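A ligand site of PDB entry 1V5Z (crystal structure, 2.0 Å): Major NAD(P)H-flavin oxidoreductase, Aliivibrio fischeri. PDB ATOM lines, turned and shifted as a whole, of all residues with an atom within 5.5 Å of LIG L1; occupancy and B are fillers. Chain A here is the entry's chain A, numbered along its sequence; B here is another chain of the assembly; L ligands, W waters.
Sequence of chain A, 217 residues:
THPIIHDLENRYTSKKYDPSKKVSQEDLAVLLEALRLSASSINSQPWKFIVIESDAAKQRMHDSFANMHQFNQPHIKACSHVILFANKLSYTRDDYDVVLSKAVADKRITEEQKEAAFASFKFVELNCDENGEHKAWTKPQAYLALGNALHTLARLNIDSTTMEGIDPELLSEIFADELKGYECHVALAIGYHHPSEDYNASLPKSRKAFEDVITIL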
ATOM      1  N   ARG A  11     -29.050 -12.485   0.181  1.00  0.00           N
ATOM      2  CA  ARG A  11     -28.471 -11.223  -0.268  1.00  0.00           C
ATOM      3  C   ARG A  11     -28.362 -10.350   0.978  1.00  0.00           C
ATOM      4  O   ARG A  11     -29.103 -10.545   1.940  1.00  0.00           O
ATOM      5  CB  ARG A  11     -29.332 -10.551  -1.346  1.00  0.00           C
ATOM      6  CG  ARG A  11     -30.736 -10.117  -0.906  1.00  0.00           C
ATOM      7  CD  ARG A  11     -31.219  -8.806  -1.569  1.00  0.00           C
ATOM      8  NE  ARG A  11     -30.356  -7.677  -1.226  1.00  0.00           N
ATOM      9  CZ  ARG A  11     -30.275  -7.108  -0.025  1.00  0.00           C
ATOM     10  NH1 ARG A  11     -31.014  -7.543   0.996  1.00  0.00           N
ATOM     11  NH2 ARG A  11     -29.381  -6.160   0.178  1.00  0.00           N
ATOM     12  N   TYR A  12     -27.376  -9.448   0.998  1.00  0.00           N
ATOM     13  CA  TYR A  12     -27.148  -8.560   2.135  1.00  0.00           C
ATOM     14  C   TYR A  12     -26.312  -7.381   1.678  1.00  0.00           C
ATOM     15  O   TYR A  12     -25.870  -7.319   0.528  1.00  0.00           O
ATOM     16  CB  TYR A  12     -26.438  -9.289   3.280  1.00  0.00           C
ATOM     17  CG  TYR A  12     -24.977  -9.565   3.018  1.00  0.00           C
ATOM     18  CD1 TYR A  12     -23.985  -8.872   3.695  1.00  0.00           C
ATOM     19  CD2 TYR A  12     -24.589 -10.457   2.010  1.00  0.00           C
ATOM     20  CE1 TYR A  12     -22.649  -9.036   3.381  1.00  0.00           C
ATOM     21  CE2 TYR A  12     -23.256 -10.630   1.697  1.00  0.00           C
ATOM     22  CZ  TYR A  12     -22.296  -9.917   2.380  1.00  0.00           C
ATOM     23  OH  TYR A  12     -20.973 -10.044   2.023  1.00  0.00           O
ATOM     24  N   THR A  13     -26.090  -6.433   2.582  1.00  0.00           N
ATOM     25  CA  THR A  13     -25.294  -5.262   2.250  1.00  0.00           C
ATOM     26  C   THR A  13     -23.835  -5.536   2.592  1.00  0.00           C
ATOM     27  O   THR A  13     -23.455  -5.682   3.757  1.00  0.00           O
ATOM     28  CB  THR A  13     -25.838  -3.994   2.964  1.00  0.00           C
ATOM     29  OG1 THR A  13     -27.158  -3.690   2.453  1.00  0.00           O
ATOM     30  CG2 THR A  13     -24.914  -2.773   2.720  1.00  0.00           C
ATOM     31  N   SER A  14     -23.014  -5.655   1.562  1.00  0.00           N
ATOM     32  CA  SER A  14     -21.592  -5.904   1.772  1.00  0.00           C
ATOM     33  C   SER A  14     -20.931  -4.666   2.383  1.00  0.00           C
ATOM     34  O   SER A  14     -21.220  -3.547   1.985  1.00  0.00           O
ATOM     35  CB  SER A  14     -20.918  -6.286   0.450  1.00  0.00           C
ATOM     36  OG  SER A  14     -19.559  -6.585   0.650  1.00  0.00           O
ATOM     37  N   LYS A  15     -20.064  -4.878   3.361  1.00  0.00           N
ATOM     38  CA  LYS A  15     -19.347  -3.805   4.051  1.00  0.00           C
ATOM     39  C   LYS A  15     -17.838  -3.786   3.754  1.00  0.00           C
ATOM     40  O   LYS A  15     -17.108  -3.032   4.372  1.00  0.00           O
ATOM     41  CB  LYS A  15     -19.556  -3.914   5.561  1.00  0.00           C
ATOM     42  CG  LYS A  15     -21.008  -3.842   6.018  1.00  0.00           C
ATOM     43  CD  LYS A  15     -21.632  -2.472   5.759  1.00  0.00           C
ATOM     44  CE  LYS A  15     -23.082  -2.419   6.228  1.00  0.00           C
ATOM     45  NZ  LYS A  15     -23.718  -1.099   5.964  1.00  0.00           N
ATOM     46  N   PHE A  71     -17.547   7.098   4.952  1.00  0.00           N
ATOM     47  CA  PHE A  71     -17.647   5.709   5.377  1.00  0.00           C
ATOM     48  C   PHE A  71     -17.947   4.822   4.156  1.00  0.00           C
ATOM     49  O   PHE A  71     -17.658   3.628   4.164  1.00  0.00           O
ATOM     50  CB  PHE A  71     -18.709   5.541   6.469  1.00  0.00           C
ATOM     51  CG  PHE A  71     -20.147   5.744   6.003  1.00  0.00           C
ATOM     52  CD1 PHE A  71     -20.980   4.651   5.774  1.00  0.00           C
ATOM     53  CD2 PHE A  71     -20.649   7.014   5.801  1.00  0.00           C
ATOM     54  CE1 PHE A  71     -22.299   4.837   5.357  1.00  0.00           C
ATOM     55  CE2 PHE A  71     -21.982   7.203   5.384  1.00  0.00           C
ATOM     56  CZ  PHE A  71     -22.794   6.106   5.163  1.00  0.00           C
ATOM     57  N   ASN A  72     -18.488   5.435   3.106  1.00  0.00           N
ATOM     58  CA  ASN A  72     -18.809   4.739   1.872  1.00  0.00           C
ATOM     59  C   ASN A  72     -17.669   4.809   0.853  1.00  0.00           C
ATOM     60  O   ASN A  72     -17.641   4.060  -0.125  1.00  0.00           O
ATOM     61  CB  ASN A  72     -20.051   5.377   1.239  1.00  0.00           C
ATOM     62  CG  ASN A  72     -21.347   4.844   1.838  1.00  0.00           C
ATOM     63  OD1 ASN A  72     -21.401   3.719   2.328  1.00  0.00           O
ATOM     64  ND2 ASN A  72     -22.393   5.653   1.785  1.00  0.00           N
ATOM     65  N   HIS A  75     -15.216   1.639  -0.696  1.00  0.00           N
ATOM     66  CA  HIS A  75     -15.838   0.686  -1.620  1.00  0.00           C
ATOM     67  C   HIS A  75     -15.619   1.031  -3.087  1.00  0.00           C
ATOM     68  O   HIS A  75     -15.618   0.137  -3.930  1.00  0.00           O
ATOM     69  CB  HIS A  75     -17.350   0.623  -1.394  1.00  0.00           C
ATOM     70  CG  HIS A  75     -17.734   0.285   0.014  1.00  0.00           C
ATOM     71  ND1 HIS A  75     -17.013  -0.592   0.782  1.00  0.00           N
ATOM     72  CD2 HIS A  75     -18.765   0.713   0.771  1.00  0.00           C
ATOM     73  CE1 HIS A  75     -17.573  -0.690   1.979  1.00  0.00           C
ATOM     74  NE2 HIS A  75     -18.642   0.084   1.991  1.00  0.00           N
ATOM     75  N   TYR A 143     -36.090   4.347  -7.795  1.00  0.00           N
ATOM     76  CA  TYR A 143     -36.003   3.437  -6.666  1.00  0.00           C
ATOM     77  C   TYR A 143     -36.653   2.102  -7.007  1.00  0.00           C
ATOM     78  O   TYR A 143     -36.244   1.062  -6.485  1.00  0.00           O
ATOM     79  CB  TYR A 143     -36.594   4.054  -5.376  1.00  0.00           C
ATOM     80  CG  TYR A 143     -35.597   4.896  -4.626  1.00  0.00           C
ATOM     81  CD1 TYR A 143     -35.082   6.068  -5.185  1.00  0.00           C
ATOM     82  CD2 TYR A 143     -35.149   4.514  -3.356  1.00  0.00           C
ATOM     83  CE1 TYR A 143     -34.145   6.835  -4.519  1.00  0.00           C
ATOM     84  CE2 TYR A 143     -34.208   5.271  -2.681  1.00  0.00           C
ATOM     85  CZ  TYR A 143     -33.707   6.441  -3.268  1.00  0.00           C
ATOM     86  OH  TYR A 143     -32.821   7.242  -2.592  1.00  0.00           O
ATOM     87  N   LEU A 146     -34.127   0.271  -8.784  1.00  0.00           N
ATOM     88  CA  LEU A 146     -33.136  -0.157  -7.799  1.00  0.00           C
ATOM     89  C   LEU A 146     -33.584  -1.443  -7.100  1.00  0.00           C
ATOM     90  O   LEU A 146     -32.764  -2.344  -6.877  1.00  0.00           O
ATOM     91  CB  LEU A 146     -32.855   0.957  -6.778  1.00  0.00           C
ATOM     92  CG  LEU A 146     -31.979   0.664  -5.554  1.00  0.00           C
ATOM     93  CD1 LEU A 146     -30.580   0.147  -5.949  1.00  0.00           C
ATOM     94  CD2 LEU A 146     -31.850   1.928  -4.699  1.00  0.00           C
ATOM     95  N   LEU A 150     -31.595  -5.036  -7.179  1.00  0.00           N
ATOM     96  CA  LEU A 150     -31.176  -5.797  -6.011  1.00  0.00           C
ATOM     97  C   LEU A 150     -31.636  -7.251  -6.093  1.00  0.00           C
ATOM     98  O   LEU A 150     -30.898  -8.156  -5.716  1.00  0.00           O
ATOM     99  CB  LEU A 150     -31.665  -5.149  -4.710  1.00  0.00           C
ATOM    100  CG  LEU A 150     -31.050  -3.804  -4.304  1.00  0.00           C
ATOM    101  CD1 LEU A 150     -31.761  -3.303  -3.054  1.00  0.00           C
ATOM    102  CD2 LEU A 150     -29.521  -3.935  -4.055  1.00  0.00           C
ATOM    103  N   THR A 161     -23.643  -2.997  -2.481  1.00  0.00           N
ATOM    104  CA  THR A 161     -23.798  -2.040  -1.392  1.00  0.00           C
ATOM    105  C   THR A 161     -24.584  -0.844  -1.936  1.00  0.00           C
ATOM    106  O   THR A 161     -24.102  -0.167  -2.827  1.00  0.00           O
ATOM    107  CB  THR A 161     -22.438  -1.518  -0.884  1.00  0.00           C
ATOM    108  OG1 THR A 161     -21.591  -2.613  -0.555  1.00  0.00           O
ATOM    109  CG2 THR A 161     -22.598  -0.644   0.364  1.00  0.00           C
ATOM    110  N   THR A 162     -25.822  -0.697  -1.479  1.00  0.00           N
ATOM    111  CA  THR A 162     -26.663   0.424  -1.885  1.00  0.00           C
ATOM    112  C   THR A 162     -26.138   1.611  -1.109  1.00  0.00           C
ATOM    113  O   THR A 162     -25.760   1.487   0.058  1.00  0.00           O
ATOM    114  CB  THR A 162     -28.164   0.192  -1.550  1.00  0.00           C
ATOM    115  OG1 THR A 162     -28.612  -1.034  -2.163  1.00  0.00           O
ATOM    116  CG2 THR A 162     -28.992   1.332  -2.111  1.00  0.00           C
ATOM    117  N   MET A 163     -26.083   2.769  -1.756  1.00  0.00           N
ATOM    118  CA  MET A 163     -25.544   3.952  -1.095  1.00  0.00           C
ATOM    119  C   MET A 163     -26.334   5.231  -1.273  1.00  0.00           C
ATOM    120  O   MET A 163     -26.478   5.738  -2.390  1.00  0.00           O
ATOM    121  CB  MET A 163     -24.088   4.176  -1.528  1.00  0.00           C
ATOM    122  CG  MET A 163     -23.101   3.094  -1.070  1.00  0.00           C
ATOM    123  SD  MET A 163     -21.387   3.265  -1.682  1.00  0.00           S
ATOM    124  CE  MET A 163     -21.739   3.428  -3.376  1.00  0.00           C
ATOM    125  N   GLU A 164     -26.905   5.710  -0.182  1.00  0.00           N
ATOM    126  CA  GLU A 164     -27.634   6.978  -0.180  1.00  0.00           C
ATOM    127  C   GLU A 164     -26.682   7.969   0.480  1.00  0.00           C
ATOM    128  O   GLU A 164     -26.916   9.180   0.459  1.00  0.00           O
ATOM    129  CB  GLU A 164     -28.948   6.873   0.614  1.00  0.00           C
ATOM    130  CG  GLU A 164     -30.193   7.021  -0.238  1.00  0.00           C
ATOM    131  CD  GLU A 164     -31.492   6.953   0.600  1.00  0.00           C
ATOM    132  OE1 GLU A 164     -31.428   7.010   1.839  1.00  0.00           O
ATOM    133  OE2 GLU A 164     -32.581   6.841   0.006  1.00  0.00           O
ATOM    134  N   GLY A 165     -25.615   7.450   1.083  1.00  0.00           N
ATOM    135  CA  GLY A 165     -24.620   8.282   1.720  1.00  0.00           C
ATOM    136  C   GLY A 165     -23.621   8.743   0.663  1.00  0.00           C
ATOM    137  O   GLY A 165     -22.473   8.341   0.674  1.00  0.00           O
ATOM    138  N   VAL A 186     -28.996   8.079  -5.161  1.00  0.00           N
ATOM    139  CA  VAL A 186     -28.570   6.768  -4.726  1.00  0.00           C
ATOM    140  C   VAL A 186     -27.625   6.091  -5.737  1.00  0.00           C
ATOM    141  O   VAL A 186     -27.752   6.264  -6.944  1.00  0.00           O
ATOM    142  CB  VAL A 186     -29.821   5.889  -4.403  1.00  0.00           C
ATOM    143  CG1 VAL A 186     -30.645   5.656  -5.632  1.00  0.00           C
ATOM    144  CG2 VAL A 186     -29.419   4.607  -3.742  1.00  0.00           C
ATOM    145  N   ASN A 200     -20.374  -7.974   7.786  1.00  0.00           N
ATOM    146  CA  ASN A 200     -21.791  -8.140   7.595  1.00  0.00           C
ATOM    147  C   ASN A 200     -22.165  -9.453   6.944  1.00  0.00           C
ATOM    148  O   ASN A 200     -23.322  -9.871   7.007  1.00  0.00           O
ATOM    149  CB  ASN A 200     -22.350  -6.972   6.803  1.00  0.00           C
ATOM    150  CG  ASN A 200     -23.768  -6.662   7.179  1.00  0.00           C
ATOM    151  OD1 ASN A 200     -24.171  -6.928   8.294  1.00  0.00           O
ATOM    152  ND2 ASN A 200     -24.534  -6.108   6.256  1.00  0.00           N
ATOM    153  N   LYS A 205     -29.691 -11.542   9.218  1.00  0.00           N
ATOM    154  CA  LYS A 205     -30.552 -10.484   8.674  1.00  0.00           C
ATOM    155  C   LYS A 205     -31.670 -10.238   9.684  1.00  0.00           C
ATOM    156  O   LYS A 205     -32.085 -11.163  10.395  1.00  0.00           O
ATOM    157  CB  LYS A 205     -31.144 -10.912   7.314  1.00  0.00           C
ATOM    158  CG  LYS A 205     -31.892  -9.805   6.569  1.00  0.00           C
ATOM    159  CD  LYS A 205     -32.370 -10.241   5.192  1.00  0.00           C
ATOM    160  CE  LYS A 205     -31.209 -10.674   4.301  1.00  0.00           C
ATOM    161  NZ  LYS A 205     -30.114  -9.681   4.272  1.00  0.00           N
ATOM    162  N   ARG A 207     -35.484  -8.206  10.183  1.00  0.00           N
ATOM    163  CA  ARG A 207     -36.596  -7.443   9.652  1.00  0.00           C
ATOM    164  C   ARG A 207     -37.677  -7.443  10.728  1.00  0.00           C
ATOM    165  O   ARG A 207     -37.639  -8.258  11.639  1.00  0.00           O
ATOM    166  CB  ARG A 207     -37.157  -8.080   8.380  1.00  0.00           C
ATOM    167  CG  ARG A 207     -36.250  -7.958   7.130  1.00  0.00           C
ATOM    168  CD  ARG A 207     -35.938  -6.499   6.734  1.00  0.00           C
ATOM    169  NE  ARG A 207     -35.241  -6.470   5.451  1.00  0.00           N
ATOM    170  CZ  ARG A 207     -33.929  -6.577   5.293  1.00  0.00           C
ATOM    171  NH1 ARG A 207     -33.156  -6.719   6.356  1.00  0.00           N
ATOM    172  NH2 ARG A 207     -33.393  -6.582   4.073  1.00  0.00           N
ATOM    173  N   LEU B  37     -38.703  -8.930   3.298  1.00  0.00           N
ATOM    174  CA  LEU B  37     -37.251  -8.993   3.213  1.00  0.00           C
ATOM    175  C   LEU B  37     -36.607  -7.867   2.406  1.00  0.00           C
ATOM    176  O   LEU B  37     -35.386  -7.798   2.348  1.00  0.00           O
ATOM    177  CB  LEU B  37     -36.818 -10.333   2.638  1.00  0.00           C
ATOM    178  CG  LEU B  37     -37.154 -11.538   3.513  1.00  0.00           C
ATOM    179  CD1 LEU B  37     -36.889 -12.821   2.711  1.00  0.00           C
ATOM    180  CD2 LEU B  37     -36.314 -11.512   4.773  1.00  0.00           C
ATOM    181  N   ALA B  39     -34.938  -4.431   1.171  1.00  0.00           N
ATOM    182  CA  ALA B  39     -33.928  -3.567   1.781  1.00  0.00           C
ATOM    183  C   ALA B  39     -34.403  -2.111   1.875  1.00  0.00           C
ATOM    184  O   ALA B  39     -35.219  -1.676   1.084  1.00  0.00           O
ATOM    185  CB  ALA B  39     -32.625  -3.666   1.003  1.00  0.00           C
ATOM    186  N   SER B  40     -33.885  -1.356   2.839  1.00  0.00           N
ATOM    187  CA  SER B  40     -34.272   0.047   2.983  1.00  0.00           C
ATOM    188  C   SER B  40     -33.170   0.747   3.720  1.00  0.00           C
ATOM    189  O   SER B  40     -32.366   0.100   4.371  1.00  0.00           O
ATOM    190  CB  SER B  40     -35.602   0.184   3.762  1.00  0.00           C
ATOM    191  OG  SER B  40     -35.516  -0.413   5.049  1.00  0.00           O
ATOM    192  N   SER B  41     -33.113   2.081   3.608  1.00  0.00           N
ATOM    193  CA  SER B  41     -32.088   2.889   4.271  1.00  0.00           C
ATOM    194  C   SER B  41     -32.137   2.623   5.753  1.00  0.00           C
ATOM    195  O   SER B  41     -33.201   2.650   6.342  1.00  0.00           O
ATOM    196  CB  SER B  41     -32.307   4.378   4.033  1.00  0.00           C
ATOM    197  OG  SER B  41     -32.622   4.608   2.678  1.00  0.00           O
ATOM    198  N   ILE B  42     -30.972   2.433   6.343  1.00  0.00           N
ATOM    199  CA  ILE B  42     -30.789   2.100   7.757  1.00  0.00           C
ATOM    200  C   ILE B  42     -31.695   0.998   8.318  1.00  0.00           C
ATOM    201  O   ILE B  42     -31.772   0.822   9.533  1.00  0.00           O
ATOM    202  CB  ILE B  42     -30.734   3.361   8.674  1.00  0.00           C
ATOM    203  CG1 ILE B  42     -32.094   4.075   8.779  1.00  0.00           C
ATOM    204  CG2 ILE B  42     -29.659   4.320   8.177  1.00  0.00           C
ATOM    205  CD1 ILE B  42     -32.097   5.149   9.848  1.00  0.00           C
ATOM    206  N   ASN B  43     -32.252   0.171   7.419  1.00  0.00           N
ATOM    207  CA  ASN B  43     -33.162  -0.928   7.770  1.00  0.00           C
ATOM    208  C   ASN B  43     -34.385  -0.329   8.474  1.00  0.00           C
ATOM    209  O   ASN B  43     -35.006  -0.950   9.324  1.00  0.00           O
ATOM    210  CB  ASN B  43     -32.476  -1.981   8.666  1.00  0.00           C
ATOM    211  CG  ASN B  43     -33.172  -3.354   8.614  1.00  0.00           C
ATOM    212  OD1 ASN B  43     -33.850  -3.675   7.647  1.00  0.00           O
ATOM    213  ND2 ASN B  43     -33.001  -4.153   9.661  1.00  0.00           N
ATOM    214  N   GLN B 141     -38.510   4.397  -0.556  1.00  0.00           N
ATOM    215  CA  GLN B 141     -38.229   3.091   0.056  1.00  0.00           C
ATOM    216  C   GLN B 141     -39.334   2.109  -0.305  1.00  0.00           C
ATOM    217  O   GLN B 141     -39.075   0.933  -0.565  1.00  0.00           O
ATOM    218  CB  GLN B 141     -38.143   3.158   1.588  1.00  0.00           C
ATOM    219  CG  GLN B 141     -37.278   4.273   2.185  1.00  0.00           C
ATOM    220  CD  GLN B 141     -35.842   4.226   1.730  1.00  0.00           C
ATOM    221  OE1 GLN B 141     -35.169   3.221   1.884  1.00  0.00           O
ATOM    222  NE2 GLN B 141     -35.364   5.332   1.163  1.00  0.00           N
ATOM    223  N   LEU B 144     -39.026   0.873  -3.794  1.00  0.00           N
ATOM    224  CA  LEU B 144     -37.981  -0.129  -3.878  1.00  0.00           C
ATOM    225  C   LEU B 144     -38.635  -1.469  -3.599  1.00  0.00           C
ATOM    226  O   LEU B 144     -38.398  -2.436  -4.315  1.00  0.00           O
ATOM    227  CB  LEU B 144     -36.883   0.154  -2.869  1.00  0.00           C
ATOM    228  CG  LEU B 144     -35.581  -0.651  -2.977  1.00  0.00           C
ATOM    229  CD1 LEU B 144     -34.501   0.079  -2.217  1.00  0.00           C
ATOM    230  CD2 LEU B 144     -35.705  -2.076  -2.444  1.00  0.00           C
HETATM  231  N1  LIG L   1     -25.564   0.858   3.477  1.00  0.00           N
HETATM  232  C1  LIG L   1     -24.303   1.380   3.485  1.00  0.00           C
HETATM  233  O1  LIG L   1     -23.391   0.885   4.133  1.00  0.00           O
HETATM  234  N2  LIG L   1     -24.292   2.697   3.120  1.00  0.00           N
HETATM  235  C2  LIG L   1     -25.349   3.447   2.589  1.00  0.00           C
HETATM  236  O2  LIG L   1     -25.109   4.628   2.283  1.00  0.00           O
HETATM  237  C3  LIG L   1     -26.590   2.761   2.567  1.00  0.00           C
HETATM  238  N3  LIG L   1     -27.674   3.425   1.988  1.00  0.00           N
HETATM  239  C4  LIG L   1     -28.821   2.759   1.699  1.00  0.00           C
HETATM  240  C5  LIG L   1     -29.738   3.320   0.845  1.00  0.00           C
HETATM  241  C6  LIG L   1     -30.872   2.619   0.498  1.00  0.00           C
HETATM  242  C7  LIG L   1     -32.015   3.237  -0.336  1.00  0.00           C
HETATM  243  C8  LIG L   1     -31.018   1.313   0.917  1.00  0.00           C
HETATM  244  C9  LIG L   1     -32.081   0.409   0.360  1.00  0.00           C
HETATM  245  C10 LIG L   1     -30.064   0.752   1.705  1.00  0.00           C
HETATM  246  C11 LIG L   1     -28.961   1.448   2.097  1.00  0.00           C
HETATM  247  N4  LIG L   1     -27.914   0.787   2.756  1.00  0.00           N
HETATM  248  C12 LIG L   1     -26.711   1.407   2.929  1.00  0.00           C
HETATM  249  C13 LIG L   1     -27.988  -0.523   3.188  1.00  0.00           C
HETATM  250  C14 LIG L   1     -29.071  -0.783   4.268  1.00  0.00           C
HETATM  251  O3  LIG L   1     -28.551  -0.542   5.550  1.00  0.00           O
HETATM  252  C15 LIG L   1     -29.554  -2.241   4.138  1.00  0.00           C
HETATM  253  O4  LIG L   1     -30.130  -2.470   2.856  1.00  0.00           O
HETATM  254  C16 LIG L   1     -30.545  -2.600   5.305  1.00  0.00           C
HETATM  255  O5  LIG L   1     -29.832  -2.467   6.586  1.00  0.00           O
HETATM  256  C17 LIG L   1     -31.051  -4.032   5.229  1.00  0.00           C
HETATM  257  O6  LIG L   1     -29.958  -5.014   5.254  1.00  0.00           O
HETATM  258  P1  LIG L   1     -29.497  -5.937   3.954  1.00  0.00           P
HETATM  259  O7  LIG L   1     -28.257  -6.395   4.597  1.00  0.00           O
HETATM  260  O8  LIG L   1     -29.425  -4.906   2.884  1.00  0.00           O
HETATM  261  O9  LIG L   1     -30.684  -6.797   3.912  1.00  0.00           O
HETATM  262  C1  LG2 L   2     -26.711   4.045   5.881  1.00  0.00           C
HETATM  263  C2  LG2 L   2     -27.027   2.536   6.178  1.00  0.00           C
HETATM  264  O1  LG2 L   2     -26.173   1.947   6.810  1.00  0.00           O
HETATM  265  O2  LG2 L   2     -28.107   2.156   5.720  1.00  0.00           O
HETATM  266  C3  LG2 L   2     -27.767   4.793   5.120  1.00  0.00           C
HETATM  267  C4  LG2 L   2     -27.561   6.264   4.762  1.00  0.00           C
HETATM  268  C5  LG2 L   2     -26.365   6.923   5.129  1.00  0.00           C
HETATM  269  C6  LG2 L   2     -26.150   8.214   4.826  1.00  0.00           C
HETATM  270  C7  LG2 L   2     -27.084   8.958   4.140  1.00  0.00           C
HETATM  271  C8  LG2 L   2     -28.360   8.359   3.715  1.00  0.00           C
HETATM  272  C9  LG2 L   2     -28.569   6.907   4.062  1.00  0.00           C
HETATM  273  O3  LG2 L   2     -29.790   6.204   3.704  1.00  0.00           O
HETATM  274  O   HOH W   1     -27.059  -4.997   6.627  1.00  0.00           O
HETATM  275  O   HOH W   2     -26.379  -2.170   6.289  1.00  0.00           O
HETATM  276  O   HOH W   3     -20.550   1.514   3.790  1.00  0.00           O
HETATM  277  O   HOH W   4     -28.598  -8.505   6.352  1.00  0.00           O
HETATM  278  O   HOH W   5     -29.503  -4.434   8.649  1.00  0.00           O
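N3 of LIG L1 sits close to O of Thr 162 (3.3 Å).
Merely in contact with LIG L1: Tyr 12 (3.5 Å), Phe 71 (3.7 Å), Tyr 143 (3.8 Å), Met 163 (3.5 Å), Ala 39 of chain B (3.3 Å), Ser 40 of chain B (3.4 Å), Ser 41 of chain B (3.4 Å), Ile 42 of chain B (3.9 Å), Asn 43 of chain B (3.4 Å), Gln 141 of chain B (3.9 Å) and Leu 144 of chain B (3.6 Å).
Within 4 Å of LIG L1: Arg 11, Tyr 12, Thr 13, Lys 15, Phe 71, Asn 72, Tyr 143, Thr 162, Met 163, Glu 164, Gly 165, Lys 205, Arg 207, Ala 39 of chain B, Ser 40 of chain B, Ser 41 of chain B, Ile 42 of chain B, Asn 43 of chain B, Gln 141 of chain B and Leu 144 of chain B.
The backbone NH (N) of Thr 13 sits at hydrogen-bond distance from an oxygen (O7) of LIG L1 (3.0 Å).
An oxygen (O8) of LIG L1 sits at hydrogen-bond distance from the side-chain hydroxyl (OG1) of Thr 13 (2.6 Å).
NZ of Lys 15 sits at hydrogen-bond distance from O1 of LIG L1.
An oxygen (O9) of LIG L1 lies within salt-bridge range of the guanidinium group (NH2) of Arg 207 (2.7 Å).
The side-chain amide nitrogen (ND2) of Asn 72 lies within hydrogen-bond range of an oxygen (O2) of LIG L1 (2.9 Å).
The side-chain amino group of Lys 205 is in salt-bridge range of an oxygen (O9) of LIG L1 (3.0 Å).
The guanidinium group (NH2) of Arg 11 lies within salt-bridge range of an oxygen (O8) of LIG L1.
The backbone NH (N) of Gly 165 sits at hydrogen-bond distance from an oxygen (O2) of LIG L1 (3.1 Å).
An oxygen (O2) of LIG L1 sits at hydrogen-bond distance from the backbone NH of Glu 164, at 3.2 Å.
OE1 of Glu 164 is in hydrogen-bond range of O3 of LG2 L2 (2.6 Å).
The side-chain hydroxyl (OG) of Ser 41 of chain B lies close to an oxygen (O3) of LG2 L2, 3.4 Å away.
The backbone NH (N) of Ile 42 of chain B sits at hydrogen-bond distance from an oxygen (O2) of LG2 L2 (2.9 Å).
Water W1 lies within hydrogen-bond range of an oxygen (O7) of LIG L1 and the side-chain amide nitrogen of Asn 200.
Water W4 lies within hydrogen-bond range of an oxygen (O7) of LIG L1 (2.8 Å) and the side-chain amino group (NZ) of Lys 205 (2.8 Å).
Water W2 bridges an oxygen (O3) of LIG L1 (2.8 Å) and the side-chain amino group of Lys 15 (2.9 Å).
Water W3 lies within hydrogen-bond range of the side-chain amide oxygen of Asn 72 (2.8 Å), an oxygen (O1) of LIG L1 (2.9 Å) and a ring nitrogen (NE2) of His 75 (3.0 Å).
O3 of LIG L1 lies within hydrogen-bond range of O2 of LG2 L2 (2.7 Å).
O of Thr 13 is in hydrogen-bond range of ND2 of Asn 200.
The side-chain amide oxygen (OD1) of Asn 43 of chain B is in hydrogen-bond range of the guanidinium group (NH1) of Arg 207 (3.4 Å).
The guanidinium group (NH2) of Arg 207 sits at hydrogen-bond distance from the backbone carbonyl oxygen (O) of Leu 37 of chain B, 2.9 Å away.
The side-chain amide nitrogen of Asn 72 lies within hydrogen-bond range of the backbone carbonyl oxygen of Gly 165 (2.9 Å).
NZ of Lys 205 sits at hydrogen-bond distance from O of Arg 11.
OH of Tyr 143 lies within hydrogen-bond range of OE2 of Glu 164 (2.6 Å).
The side-chain amide nitrogen (NE2) of Gln 141 of chain B sits at hydrogen-bond distance from the side-chain carboxylate (OE2) of Glu 164.
N of Ser 41 of chain B sits at hydrogen-bond distance from OE1 of Gln 141 of chain B.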
